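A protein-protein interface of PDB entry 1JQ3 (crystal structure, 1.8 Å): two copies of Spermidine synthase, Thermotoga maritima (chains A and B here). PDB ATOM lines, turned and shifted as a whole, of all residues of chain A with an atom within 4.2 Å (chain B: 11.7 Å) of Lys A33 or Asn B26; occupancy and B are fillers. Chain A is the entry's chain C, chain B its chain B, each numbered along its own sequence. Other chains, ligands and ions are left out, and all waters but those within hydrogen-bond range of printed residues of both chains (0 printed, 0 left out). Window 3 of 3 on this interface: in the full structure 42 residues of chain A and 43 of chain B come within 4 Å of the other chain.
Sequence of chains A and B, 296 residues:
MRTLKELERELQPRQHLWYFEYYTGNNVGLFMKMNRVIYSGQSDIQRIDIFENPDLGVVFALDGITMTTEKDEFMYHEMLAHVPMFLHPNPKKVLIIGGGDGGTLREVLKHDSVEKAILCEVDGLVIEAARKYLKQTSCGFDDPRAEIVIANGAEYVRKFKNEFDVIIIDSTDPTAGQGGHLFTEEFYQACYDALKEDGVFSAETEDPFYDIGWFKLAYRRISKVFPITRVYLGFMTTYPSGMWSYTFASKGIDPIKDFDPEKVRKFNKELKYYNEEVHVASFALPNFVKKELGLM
No position is printed for both chains.
Of the 7 pairs that touch across the chains among the printed residues, none has its exchanged pair printed and touching as well.
The backbone carbonyl oxygen of Gly B25 is in hydrogen-bond range of the side-chain amide nitrogen of Asn B27 (3.4 Å).
The backbone carbonyl oxygen (O) of Val B28 lies within hydrogen-bond range of the backbone NH (N) of Tyr B23 (2.9 Å).
The backbone carbonyl oxygen (O) of Lys A33 lies within hydrogen-bond range of the side-chain amide nitrogen (ND2) of Asn A53, at 2.8 Å.
The backbone carbonyl oxygen of Gln A15 is in hydrogen-bond range of the indole nitrogen of Trp A18 (2.8 Å).
Of the 12 printed residues of chain A, 5 touch a printed residue of chain B.
Printed residues of chain A that touch a printed residue of chain B: Trp A18, Met A32, Lys A33, Asn A53 and Pro A54.
Hydrophobic or aromatic side chains of chain A that line the printed part of chain B: Trp A18 and Pro A54.
Of the 22 printed residues of chain B, 3 touch a printed residue of chain A.
Among the printed residues, no Asp or Glu carboxylate lies within 4 Å of a Lys or Arg side-chain nitrogen of the other chain.
No residue of chain B comes within 4 Å of Pro A13.
Gln A15 touches none of the printed residues of chain B.
Trp A18 touches just one residue of chain B: Asn B26 (3.97 Å).
Of chain B, only Asn B27 comes within 4 Å of Met A32.
Lys A33 touches two residues of chain B.
Of chain B, only Asn B27 and Val B28 come within 4 Å of Asn A53.
Of the printed residues of chain B, Pro A54 touches Asn B27.
Of chain A, only Trp A18 and Lys A33 come within 4 Å of Asn B26.
Printed residues of chain A within 4 Å of Val B28: Asn A53 (3.8 Å).
O of Asn B27 is in hydrogen-bond range of ND2 of Asn A53 (3.0 Å).
The backbone carbonyl oxygen of Asn B27 lies within hydrogen-bond range of the backbone NH of Lys A33 (2.9 Å).
The backbone carbonyl oxygen of Asn B26 lies within hydrogen-bond range of the side-chain amino group of Lys A33 (3.4 Å).
CH2 of Trp A18 touches O of Asn B26 (3.97 Å).
O of Asn B27 touches CA of Met A32 (3.6 Å).
OD1 of Asn A53 touches CG2 of Val B28, at 3.8 Å.
Pro A54 touches Asn B27 (CB to CG, 3.7 Å).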
ATOM      1  N   PRO A  13     -32.904   6.231 -25.295  1.00  0.00           N
ATOM      2  CA  PRO A  13     -32.474   5.637 -24.026  1.00  0.00           C
ATOM      3  C   PRO A  13     -32.683   6.524 -22.807  1.00  0.00           C
ATOM      4  O   PRO A  13     -32.504   7.741 -22.873  1.00  0.00           O
ATOM      5  CB  PRO A  13     -30.981   5.397 -24.261  1.00  0.00           C
ATOM      6  CG  PRO A  13     -30.590   6.574 -25.108  1.00  0.00           C
ATOM      7  CD  PRO A  13     -31.743   6.647 -26.108  1.00  0.00           C
ATOM      8  N   ARG A  14     -33.038   5.905 -21.688  1.00  0.00           N
ATOM      9  CA  ARG A  14     -33.220   6.635 -20.441  1.00  0.00           C
ATOM     10  C   ARG A  14     -32.242   6.036 -19.428  1.00  0.00           C
ATOM     11  O   ARG A  14     -31.238   5.462 -19.832  1.00  0.00           O
ATOM     12  CB  ARG A  14     -34.671   6.541 -19.966  1.00  0.00           C
ATOM     13  CG  ARG A  14     -35.662   6.987 -21.038  1.00  0.00           C
ATOM     14  CD  ARG A  14     -37.082   7.085 -20.519  1.00  0.00           C
ATOM     15  NE  ARG A  14     -37.255   8.212 -19.608  1.00  0.00           N
ATOM     16  CZ  ARG A  14     -37.454   9.473 -19.990  1.00  0.00           C
ATOM     17  NH1 ARG A  14     -37.513   9.794 -21.279  1.00  0.00           N
ATOM     18  NH2 ARG A  14     -37.584  10.423 -19.076  1.00  0.00           N
ATOM     19  N   GLN A  15     -32.524   6.145 -18.133  1.00  0.00           N
ATOM     20  CA  GLN A  15     -31.610   5.615 -17.119  1.00  0.00           C
ATOM     21  C   GLN A  15     -32.212   4.460 -16.323  1.00  0.00           C
ATOM     22  O   GLN A  15     -31.764   4.167 -15.212  1.00  0.00           O
ATOM     23  CB  GLN A  15     -31.190   6.731 -16.153  1.00  0.00           C
ATOM     24  CG  GLN A  15     -30.254   7.793 -16.754  1.00  0.00           C
ATOM     25  CD  GLN A  15     -30.941   8.694 -17.770  1.00  0.00           C
ATOM     26  OE1 GLN A  15     -30.423   8.919 -18.863  1.00  0.00           O
ATOM     27  NE2 GLN A  15     -32.114   9.215 -17.409  1.00  0.00           N
ATOM     28  N   LEU A  17     -32.889   1.003 -17.747  1.00  0.00           N
ATOM     29  CA  LEU A  17     -32.545  -0.366 -18.151  1.00  0.00           C
ATOM     30  C   LEU A  17     -31.039  -0.571 -18.144  1.00  0.00           C
ATOM     31  O   LEU A  17     -30.287   0.188 -18.785  1.00  0.00           O
ATOM     32  CB  LEU A  17     -33.110  -0.707 -19.533  1.00  0.00           C
ATOM     33  CG  LEU A  17     -34.629  -0.567 -19.719  1.00  0.00           C
ATOM     34  CD1 LEU A  17     -34.984  -1.034 -21.119  1.00  0.00           C
ATOM     35  CD2 LEU A  17     -35.397  -1.371 -18.678  1.00  0.00           C
ATOM     36  N   TRP A  18     -30.613  -1.632 -17.461  1.00  0.00           N
ATOM     37  CA  TRP A  18     -29.178  -1.912 -17.321  1.00  0.00           C
ATOM     38  C   TRP A  18     -28.770  -3.380 -17.402  1.00  0.00           C
ATOM     39  O   TRP A  18     -29.512  -4.261 -17.012  1.00  0.00           O
ATOM     40  CB  TRP A  18     -28.691  -1.365 -15.969  1.00  0.00           C
ATOM     41  CG  TRP A  18     -28.925   0.112 -15.789  1.00  0.00           C
ATOM     42  CD1 TRP A  18     -30.038   0.710 -15.251  1.00  0.00           C
ATOM     43  CD2 TRP A  18     -28.062   1.175 -16.206  1.00  0.00           C
ATOM     44  NE1 TRP A  18     -29.923   2.078 -15.323  1.00  0.00           N
ATOM     45  CE2 TRP A  18     -28.722   2.393 -15.903  1.00  0.00           C
ATOM     46  CE3 TRP A  18     -26.800   1.222 -16.815  1.00  0.00           C
ATOM     47  CZ2 TRP A  18     -28.159   3.641 -16.190  1.00  0.00           C
ATOM     48  CZ3 TRP A  18     -26.241   2.467 -17.103  1.00  0.00           C
ATOM     49  CH2 TRP A  18     -26.924   3.659 -16.790  1.00  0.00           C
ATOM     50  N   MET A  32     -23.740  -1.613 -18.262  1.00  0.00           N
ATOM     51  CA  MET A  32     -24.026  -0.971 -19.538  1.00  0.00           C
ATOM     52  C   MET A  32     -25.495  -0.625 -19.637  1.00  0.00           C
ATOM     53  O   MET A  32     -26.358  -1.419 -19.249  1.00  0.00           O
ATOM     54  CB  MET A  32     -23.713  -1.915 -20.702  1.00  0.00           C
ATOM     55  CG  MET A  32     -22.266  -2.339 -20.837  1.00  0.00           C
ATOM     56  SD  MET A  32     -22.233  -3.474 -22.238  1.00  0.00           S
ATOM     57  CE  MET A  32     -20.556  -4.071 -22.155  1.00  0.00           C
ATOM     58  N   LYS A  33     -25.764   0.566 -20.153  1.00  0.00           N
ATOM     59  CA  LYS A  33     -27.133   1.043 -20.364  1.00  0.00           C
ATOM     60  C   LYS A  33     -27.694   0.283 -21.564  1.00  0.00           C
ATOM     61  O   LYS A  33     -26.965   0.001 -22.525  1.00  0.00           O
ATOM     62  CB  LYS A  33     -27.108   2.541 -20.688  1.00  0.00           C
ATOM     63  CG  LYS A  33     -28.479   3.175 -20.944  1.00  0.00           C
ATOM     64  CD  LYS A  33     -28.363   4.691 -21.165  1.00  0.00           C
ATOM     65  CE  LYS A  33     -27.982   5.426 -19.896  1.00  0.00           C
ATOM     66  NZ  LYS A  33     -27.854   6.898 -20.156  1.00  0.00           N
ATOM     67  N   MET A  34     -28.970  -0.086 -21.505  1.00  0.00           N
ATOM     68  CA  MET A  34     -29.593  -0.778 -22.640  1.00  0.00           C
ATOM     69  C   MET A  34     -30.711   0.087 -23.229  1.00  0.00           C
ATOM     70  O   MET A  34     -31.674   0.424 -22.531  1.00  0.00           O
ATOM     71  CB  MET A  34     -30.217  -2.106 -22.202  1.00  0.00           C
ATOM     72  CG  MET A  34     -29.279  -3.004 -21.419  1.00  0.00           C
ATOM     73  SD  MET A  34     -29.886  -4.703 -21.319  1.00  0.00           S
ATOM     74  CE  MET A  34     -31.393  -4.500 -20.289  1.00  0.00           C
ATOM     75  N   ASN A  35     -30.588   0.441 -24.504  1.00  0.00           N
ATOM     76  CA  ASN A  35     -31.656   1.216 -25.139  1.00  0.00           C
ATOM     77  C   ASN A  35     -32.797   0.252 -25.467  1.00  0.00           C
ATOM     78  O   ASN A  35     -33.974   0.612 -25.419  1.00  0.00           O
ATOM     79  CB  ASN A  35     -31.182   1.897 -26.413  1.00  0.00           C
ATOM     80  CG  ASN A  35     -32.241   2.811 -26.981  1.00  0.00           C
ATOM     81  OD1 ASN A  35     -32.950   3.470 -26.223  1.00  0.00           O
ATOM     82  ND2 ASN A  35     -32.382   2.830 -28.312  1.00  0.00           N
ATOM     83  N   GLU A  52     -28.818  -3.399 -27.240  1.00  0.00           N
ATOM     84  CA  GLU A  52     -28.216  -2.226 -27.830  1.00  0.00           C
ATOM     85  C   GLU A  52     -27.804  -1.229 -26.753  1.00  0.00           C
ATOM     86  O   GLU A  52     -28.598  -0.897 -25.873  1.00  0.00           O
ATOM     87  CB  GLU A  52     -29.250  -1.603 -28.775  1.00  0.00           C
ATOM     88  CG  GLU A  52     -28.903  -0.293 -29.433  1.00  0.00           C
ATOM     89  CD  GLU A  52     -30.116   0.275 -30.159  1.00  0.00           C
ATOM     90  OE1 GLU A  52     -30.472   1.448 -29.919  1.00  0.00           O
ATOM     91  OE2 GLU A  52     -30.733  -0.480 -30.954  1.00  0.00           O
ATOM     92  N   ASN A  53     -26.547  -0.799 -26.809  1.00  0.00           N
ATOM     93  CA  ASN A  53     -26.011   0.200 -25.877  1.00  0.00           C
ATOM     94  C   ASN A  53     -25.685   1.420 -26.737  1.00  0.00           C
ATOM     95  O   ASN A  53     -25.144   1.280 -27.841  1.00  0.00           O
ATOM     96  CB  ASN A  53     -24.753  -0.334 -25.183  1.00  0.00           C
ATOM     97  CG  ASN A  53     -24.027   0.735 -24.363  1.00  0.00           C
ATOM     98  OD1 ASN A  53     -23.165   1.439 -24.877  1.00  0.00           O
ATOM     99  ND2 ASN A  53     -24.399   0.873 -23.097  1.00  0.00           N
ATOM    100  N   PRO A  54     -26.016   2.631 -26.251  1.00  0.00           N
ATOM    101  CA  PRO A  54     -25.762   3.878 -26.986  1.00  0.00           C
ATOM    102  C   PRO A  54     -24.328   4.103 -27.485  1.00  0.00           C
ATOM    103  O   PRO A  54     -24.123   4.667 -28.560  1.00  0.00           O
ATOM    104  CB  PRO A  54     -26.192   4.952 -25.978  1.00  0.00           C
ATOM    105  CG  PRO A  54     -27.318   4.288 -25.259  1.00  0.00           C
ATOM    106  CD  PRO A  54     -26.698   2.918 -24.973  1.00  0.00           C
ATOM    107  N   TYR B  19     -19.907   1.055  -5.262  1.00  0.00           N
ATOM    108  CA  TYR B  19     -19.327   2.237  -5.865  1.00  0.00           C
ATOM    109  C   TYR B  19     -19.561   2.057  -7.362  1.00  0.00           C
ATOM    110  O   TYR B  19     -19.232   0.999  -7.908  1.00  0.00           O
ATOM    111  CB  TYR B  19     -17.819   2.272  -5.613  1.00  0.00           C
ATOM    112  CG  TYR B  19     -17.064   3.222  -6.516  1.00  0.00           C
ATOM    113  CD1 TYR B  19     -17.142   4.610  -6.335  1.00  0.00           C
ATOM    114  CD2 TYR B  19     -16.218   2.734  -7.508  1.00  0.00           C
ATOM    115  CE1 TYR B  19     -16.376   5.489  -7.118  1.00  0.00           C
ATOM    116  CE2 TYR B  19     -15.446   3.600  -8.301  1.00  0.00           C
ATOM    117  CZ  TYR B  19     -15.523   4.975  -8.103  1.00  0.00           C
ATOM    118  OH  TYR B  19     -14.732   5.802  -8.877  1.00  0.00           O
ATOM    119  N   PHE B  20     -20.197   3.047  -7.994  1.00  0.00           N
ATOM    120  CA  PHE B  20     -20.462   3.031  -9.440  1.00  0.00           C
ATOM    121  C   PHE B  20     -19.677   4.171 -10.081  1.00  0.00           C
ATOM    122  O   PHE B  20     -19.891   5.344  -9.738  1.00  0.00           O
ATOM    123  CB  PHE B  20     -21.947   3.324  -9.743  1.00  0.00           C
ATOM    124  CG  PHE B  20     -22.896   2.205  -9.423  1.00  0.00           C
ATOM    125  CD1 PHE B  20     -22.493   1.070  -8.739  1.00  0.00           C
ATOM    126  CD2 PHE B  20     -24.227   2.293  -9.839  1.00  0.00           C
ATOM    127  CE1 PHE B  20     -23.397   0.029  -8.478  1.00  0.00           C
ATOM    128  CE2 PHE B  20     -25.130   1.265  -9.583  1.00  0.00           C
ATOM    129  CZ  PHE B  20     -24.706   0.127  -8.899  1.00  0.00           C
ATOM    130  N   GLU B  21     -18.802   3.836 -11.030  1.00  0.00           N
ATOM    131  CA  GLU B  21     -18.038   4.849 -11.744  1.00  0.00           C
ATOM    132  C   GLU B  21     -18.595   4.965 -13.151  1.00  0.00           C
ATOM    133  O   GLU B  21     -18.492   4.026 -13.945  1.00  0.00           O
ATOM    134  CB  GLU B  21     -16.544   4.495 -11.831  1.00  0.00           C
ATOM    135  CG  GLU B  21     -15.770   5.506 -12.693  1.00  0.00           C
ATOM    136  CD  GLU B  21     -14.312   5.168 -12.893  1.00  0.00           C
ATOM    137  OE1 GLU B  21     -13.940   3.985 -12.755  1.00  0.00           O
ATOM    138  OE2 GLU B  21     -13.547   6.090 -13.242  1.00  0.00           O
ATOM    139  N   TYR B  22     -19.208   6.102 -13.460  1.00  0.00           N
ATOM    140  CA  TYR B  22     -19.761   6.302 -14.802  1.00  0.00           C
ATOM    141  C   TYR B  22     -18.703   6.840 -15.755  1.00  0.00           C
ATOM    142  O   TYR B  22     -17.944   7.746 -15.412  1.00  0.00           O
ATOM    143  CB  TYR B  22     -20.964   7.260 -14.767  1.00  0.00           C
ATOM    144  CG  TYR B  22     -22.174   6.693 -14.073  1.00  0.00           C
ATOM    145  CD1 TYR B  22     -22.294   6.745 -12.681  1.00  0.00           C
ATOM    146  CD2 TYR B  22     -23.190   6.072 -14.799  1.00  0.00           C
ATOM    147  CE1 TYR B  22     -23.396   6.186 -12.025  1.00  0.00           C
ATOM    148  CE2 TYR B  22     -24.288   5.512 -14.160  1.00  0.00           C
ATOM    149  CZ  TYR B  22     -24.386   5.571 -12.772  1.00  0.00           C
ATOM    150  OH  TYR B  22     -25.460   4.995 -12.135  1.00  0.00           O
ATOM    151  N   TYR B  23     -18.629   6.265 -16.953  1.00  0.00           N
ATOM    152  CA  TYR B  23     -17.673   6.736 -17.941  1.00  0.00           C
ATOM    153  C   TYR B  23     -18.272   7.898 -18.721  1.00  0.00           C
ATOM    154  O   TYR B  23     -19.467   8.160 -18.625  1.00  0.00           O
ATOM    155  CB  TYR B  23     -17.318   5.617 -18.910  1.00  0.00           C
ATOM    156  CG  TYR B  23     -16.671   4.446 -18.224  1.00  0.00           C
ATOM    157  CD1 TYR B  23     -16.027   4.598 -16.987  1.00  0.00           C
ATOM    158  CD2 TYR B  23     -16.661   3.191 -18.827  1.00  0.00           C
ATOM    159  CE1 TYR B  23     -15.376   3.517 -16.377  1.00  0.00           C
ATOM    160  CE2 TYR B  23     -16.020   2.112 -18.225  1.00  0.00           C
ATOM    161  CZ  TYR B  23     -15.375   2.282 -17.013  1.00  0.00           C
ATOM    162  OH  TYR B  23     -14.666   1.217 -16.491  1.00  0.00           O
ATOM    163  N   THR B  24     -17.425   8.587 -19.480  1.00  0.00           N
ATOM    164  CA  THR B  24     -17.853   9.717 -20.295  1.00  0.00           C
ATOM    165  C   THR B  24     -19.000   9.250 -21.178  1.00  0.00           C
ATOM    166  O   THR B  24     -18.886   8.243 -21.891  1.00  0.00           O
ATOM    167  CB  THR B  24     -16.678  10.257 -21.158  1.00  0.00           C
ATOM    168  OG1 THR B  24     -15.644  10.736 -20.291  1.00  0.00           O
ATOM    169  CG2 THR B  24     -17.129  11.412 -22.057  1.00  0.00           C
ATOM    170  N   GLY B  25     -20.133   9.935 -21.040  1.00  0.00           N
ATOM    171  CA  GLY B  25     -21.323   9.603 -21.802  1.00  0.00           C
ATOM    172  C   GLY B  25     -22.410   9.025 -20.913  1.00  0.00           C
ATOM    173  O   GLY B  25     -23.592   9.058 -21.264  1.00  0.00           O
ATOM    174  N   ASN B  26     -21.999   8.467 -19.776  1.00  0.00           N
ATOM    175  CA  ASN B  26     -22.907   7.863 -18.800  1.00  0.00           C
ATOM    176  C   ASN B  26     -23.685   6.653 -19.329  1.00  0.00           C
ATOM    177  O   ASN B  26     -24.742   6.299 -18.801  1.00  0.00           O
ATOM    178  CB  ASN B  26     -23.860   8.918 -18.232  1.00  0.00           C
ATOM    179  CG  ASN B  26     -23.124  10.026 -17.497  1.00  0.00           C
ATOM    180  OD1 ASN B  26     -22.142   9.778 -16.790  1.00  0.00           O
ATOM    181  ND2 ASN B  26     -23.598  11.259 -17.656  1.00  0.00           N
ATOM    182  N   ASN B  27     -23.129   6.002 -20.345  1.00  0.00           N
ATOM    183  CA  ASN B  27     -23.739   4.825 -20.955  1.00  0.00           C
ATOM    184  C   ASN B  27     -23.089   3.506 -20.512  1.00  0.00           C
ATOM    185  O   ASN B  27     -23.670   2.439 -20.701  1.00  0.00           O
ATOM    186  CB  ASN B  27     -23.680   4.933 -22.481  1.00  0.00           C
ATOM    187  CG  ASN B  27     -24.440   6.139 -23.003  1.00  0.00           C
ATOM    188  OD1 ASN B  27     -25.582   6.370 -22.611  1.00  0.00           O
ATOM    189  ND2 ASN B  27     -23.796   6.934 -23.857  1.00  0.00           N
ATOM    190  N   VAL B  28     -21.868   3.590 -19.978  1.00  0.00           N
ATOM    191  CA  VAL B  28     -21.109   2.421 -19.521  1.00  0.00           C
ATOM    192  C   VAL B  28     -20.340   2.842 -18.269  1.00  0.00           C
ATOM    193  O   VAL B  28     -20.096   4.032 -18.056  1.00  0.00           O
ATOM    194  CB  VAL B  28     -20.065   1.978 -20.583  1.00  0.00           C
ATOM    195  CG1 VAL B  28     -19.262   0.768 -20.095  1.00  0.00           C
ATOM    196  CG2 VAL B  28     -20.763   1.635 -21.899  1.00  0.00           C
ATOM    197  N   GLY B  29     -19.978   1.873 -17.435  1.00  0.00           N
ATOM    198  CA  GLY B  29     -19.229   2.196 -16.237  1.00  0.00           C
ATOM    199  C   GLY B  29     -18.755   0.965 -15.506  1.00  0.00           C
ATOM    200  O   GLY B  29     -19.049  -0.168 -15.902  1.00  0.00           O
ATOM    201  N   LEU B  30     -18.004   1.191 -14.439  1.00  0.00           N
ATOM    202  CA  LEU B  30     -17.466   0.106 -13.636  1.00  0.00           C
ATOM    203  C   LEU B  30     -18.095   0.152 -12.249  1.00  0.00           C
ATOM    204  O   LEU B  30     -18.375   1.240 -11.734  1.00  0.00           O
ATOM    205  CB  LEU B  30     -15.954   0.316 -13.479  1.00  0.00           C
ATOM    206  CG  LEU B  30     -15.147  -0.887 -12.970  1.00  0.00           C
ATOM    207  CD1 LEU B  30     -14.924  -1.860 -14.130  1.00  0.00           C
ATOM    208  CD2 LEU B  30     -13.809  -0.413 -12.423  1.00  0.00           C
ATOM    209  N   PHE B  31     -18.372  -1.014 -11.664  1.00  0.00           N
ATOM    210  CA  PHE B  31     -18.911  -1.039 -10.310  1.00  0.00           C
ATOM    211  C   PHE B  31     -17.971  -1.848  -9.422  1.00  0.00           C
ATOM    212  O   PHE B  31     -17.282  -2.765  -9.887  1.00  0.00           O
ATOM    213  CB  PHE B  31     -20.361  -1.557 -10.243  1.00  0.00           C
ATOM    214  CG  PHE B  31     -20.542  -2.983 -10.667  1.00  0.00           C
ATOM    215  CD1 PHE B  31     -20.502  -4.010  -9.733  1.00  0.00           C
ATOM    216  CD2 PHE B  31     -20.892  -3.287 -11.974  1.00  0.00           C
ATOM    217  CE1 PHE B  31     -20.821  -5.311 -10.086  1.00  0.00           C
ATOM    218  CE2 PHE B  31     -21.216  -4.593 -12.340  1.00  0.00           C
ATOM    219  CZ  PHE B  31     -21.183  -5.603 -11.395  1.00  0.00           C
ATOM    220  N   ASP B  63     -14.491  12.918  -7.245  1.00  0.00           N
ATOM    221  CA  ASP B  63     -15.763  13.214  -7.921  1.00  0.00           C
ATOM    222  C   ASP B  63     -16.349  11.967  -8.593  1.00  0.00           C
ATOM    223  O   ASP B  63     -16.922  12.040  -9.680  1.00  0.00           O
ATOM    224  CB  ASP B  63     -15.589  14.351  -8.934  1.00  0.00           C
ATOM    225  CG  ASP B  63     -15.506  15.718  -8.263  1.00  0.00           C
ATOM    226  OD1 ASP B  63     -15.813  15.814  -7.054  1.00  0.00           O
ATOM    227  OD2 ASP B  63     -15.121  16.687  -8.950  1.00  0.00           O
ATOM    228  N   GLY B  64     -16.225  10.829  -7.921  1.00  0.00           N
ATOM    229  CA  GLY B  64     -16.757   9.584  -8.459  1.00  0.00           C
ATOM    230  C   GLY B  64     -16.026   9.013  -9.663  1.00  0.00           C
ATOM    231  O   GLY B  64     -16.609   8.265 -10.470  1.00  0.00           O
ATOM    232  N   ILE B  65     -14.766   9.393  -9.812  1.00  0.00           N
ATOM    233  CA  ILE B  65     -13.926   8.902 -10.896  1.00  0.00           C
ATOM    234  C   ILE B  65     -12.764   8.177 -10.220  1.00  0.00           C
ATOM    235  O   ILE B  65     -12.133   8.722  -9.325  1.00  0.00           O
ATOM    236  CB  ILE B  65     -13.419  10.077 -11.768  1.00  0.00           C
ATOM    237  CG1 ILE B  65     -14.614  10.745 -12.468  1.00  0.00           C
ATOM    238  CG2 ILE B  65     -12.444   9.583 -12.812  1.00  0.00           C
ATOM    239  CD1 ILE B  65     -14.246  11.968 -13.299  1.00  0.00           C
ATOM    240  N   ASP B 207      -7.925   7.504 -22.439  1.00  0.00           N
ATOM    241  CA  ASP B 207      -8.205   6.334 -23.262  1.00  0.00           C
ATOM    242  C   ASP B 207      -8.747   6.775 -24.616  1.00  0.00           C
ATOM    243  O   ASP B 207      -9.662   7.609 -24.690  1.00  0.00           O
ATOM    244  CB  ASP B 207      -9.265   5.441 -22.591  1.00  0.00           C
ATOM    245  CG  ASP B 207     -10.551   6.200 -22.250  1.00  0.00           C
ATOM    246  OD1 ASP B 207     -10.522   7.094 -21.373  1.00  0.00           O
ATOM    247  OD2 ASP B 207     -11.603   5.869 -22.841  1.00  0.00           O
ATOM    248  N   PHE B 209     -10.856   5.735 -26.469  1.00  0.00           N
ATOM    249  CA  PHE B 209     -12.095   4.964 -26.629  1.00  0.00           C
ATOM    250  C   PHE B 209     -13.221   5.883 -26.150  1.00  0.00           C
ATOM    251  O   PHE B 209     -13.763   6.653 -26.948  1.00  0.00           O
ATOM    252  CB  PHE B 209     -12.033   3.659 -25.795  1.00  0.00           C
ATOM    253  CG  PHE B 209     -13.044   2.605 -26.213  1.00  0.00           C
ATOM    254  CD1 PHE B 209     -12.986   2.026 -27.484  1.00  0.00           C
ATOM    255  CD2 PHE B 209     -14.064   2.220 -25.350  1.00  0.00           C
ATOM    256  CE1 PHE B 209     -13.938   1.084 -27.892  1.00  0.00           C
ATOM    257  CE2 PHE B 209     -15.034   1.265 -25.745  1.00  0.00           C
ATOM    258  CZ  PHE B 209     -14.966   0.705 -27.019  1.00  0.00           C
ATOM    259  N   TYR B 210     -13.517   5.881 -24.851  1.00  0.00           N
ATOM    260  CA  TYR B 210     -14.568   6.764 -24.324  1.00  0.00           C
ATOM    261  C   TYR B 210     -14.181   8.245 -24.363  1.00  0.00           C
ATOM    262  O   TYR B 210     -15.042   9.131 -24.463  1.00  0.00           O
ATOM    263  CB  TYR B 210     -14.897   6.411 -22.870  1.00  0.00           C
ATOM    264  CG  TYR B 210     -15.407   5.003 -22.706  1.00  0.00           C
ATOM    265  CD1 TYR B 210     -16.642   4.632 -23.235  1.00  0.00           C
ATOM    266  CD2 TYR B 210     -14.647   4.033 -22.039  1.00  0.00           C
ATOM    267  CE1 TYR B 210     -17.113   3.351 -23.111  1.00  0.00           C
ATOM    268  CE2 TYR B 210     -15.110   2.730 -21.913  1.00  0.00           C
ATOM    269  CZ  TYR B 210     -16.347   2.398 -22.457  1.00  0.00           C
ATOM    270  OH  TYR B 210     -16.790   1.101 -22.389  1.00  0.00           O
ATOM    271  N   ASP B 211     -12.886   8.512 -24.274  1.00  0.00           N
ATOM    272  CA  ASP B 211     -12.403   9.889 -24.242  1.00  0.00           C
ATOM    273  C   ASP B 211     -11.576  10.256 -25.463  1.00  0.00           C
ATOM    274  O   ASP B 211     -10.622  11.032 -25.382  1.00  0.00           O
ATOM    275  CB  ASP B 211     -11.618  10.091 -22.943  1.00  0.00           C
ATOM    276  CG  ASP B 211     -12.486   9.862 -21.707  1.00  0.00           C
ATOM    277  OD1 ASP B 211     -12.484   8.742 -21.135  1.00  0.00           O
ATOM    278  OD2 ASP B 211     -13.211  10.799 -21.323  1.00  0.00           O
ATOM    279  N   TRP B 214     -10.929  14.147 -26.327  1.00  0.00           N
ATOM    280  CA  TRP B 214      -9.878  14.765 -25.537  1.00  0.00           C
ATOM    281  C   TRP B 214      -8.501  14.213 -25.873  1.00  0.00           C
ATOM    282  O   TRP B 214      -7.527  14.956 -25.853  1.00  0.00           O
ATOM    283  CB  TRP B 214     -10.181  14.605 -24.046  1.00  0.00           C
ATOM    284  CG  TRP B 214     -11.561  15.073 -23.706  1.00  0.00           C
ATOM    285  CD1 TRP B 214     -12.692  14.301 -23.614  1.00  0.00           C
ATOM    286  CD2 TRP B 214     -11.982  16.429 -23.483  1.00  0.00           C
ATOM    287  NE1 TRP B 214     -13.789  15.097 -23.358  1.00  0.00           N
ATOM    288  CE2 TRP B 214     -13.383  16.404 -23.274  1.00  0.00           C
ATOM    289  CE3 TRP B 214     -11.312  17.662 -23.448  1.00  0.00           C
ATOM    290  CZ2 TRP B 214     -14.128  17.568 -23.031  1.00  0.00           C
ATOM    291  CZ3 TRP B 214     -12.051  18.816 -23.208  1.00  0.00           C
ATOM    292  CH2 TRP B 214     -13.448  18.759 -23.002  1.00  0.00           C
ATOM    293  N   PRO B 240     -11.056   3.585 -17.308  1.00  0.00           N
ATOM    294  CA  PRO B 240     -12.023   3.378 -18.386  1.00  0.00           C
ATOM    295  C   PRO B 240     -11.423   2.767 -19.663  1.00  0.00           C
ATOM    296  O   PRO B 240     -10.537   3.341 -20.294  1.00  0.00           O
ATOM    297  CB  PRO B 240     -12.587   4.785 -18.623  1.00  0.00           C
ATOM    298  CG  PRO B 240     -12.390   5.493 -17.264  1.00  0.00           C
ATOM    299  CD  PRO B 240     -11.033   4.990 -16.851  1.00  0.00           C
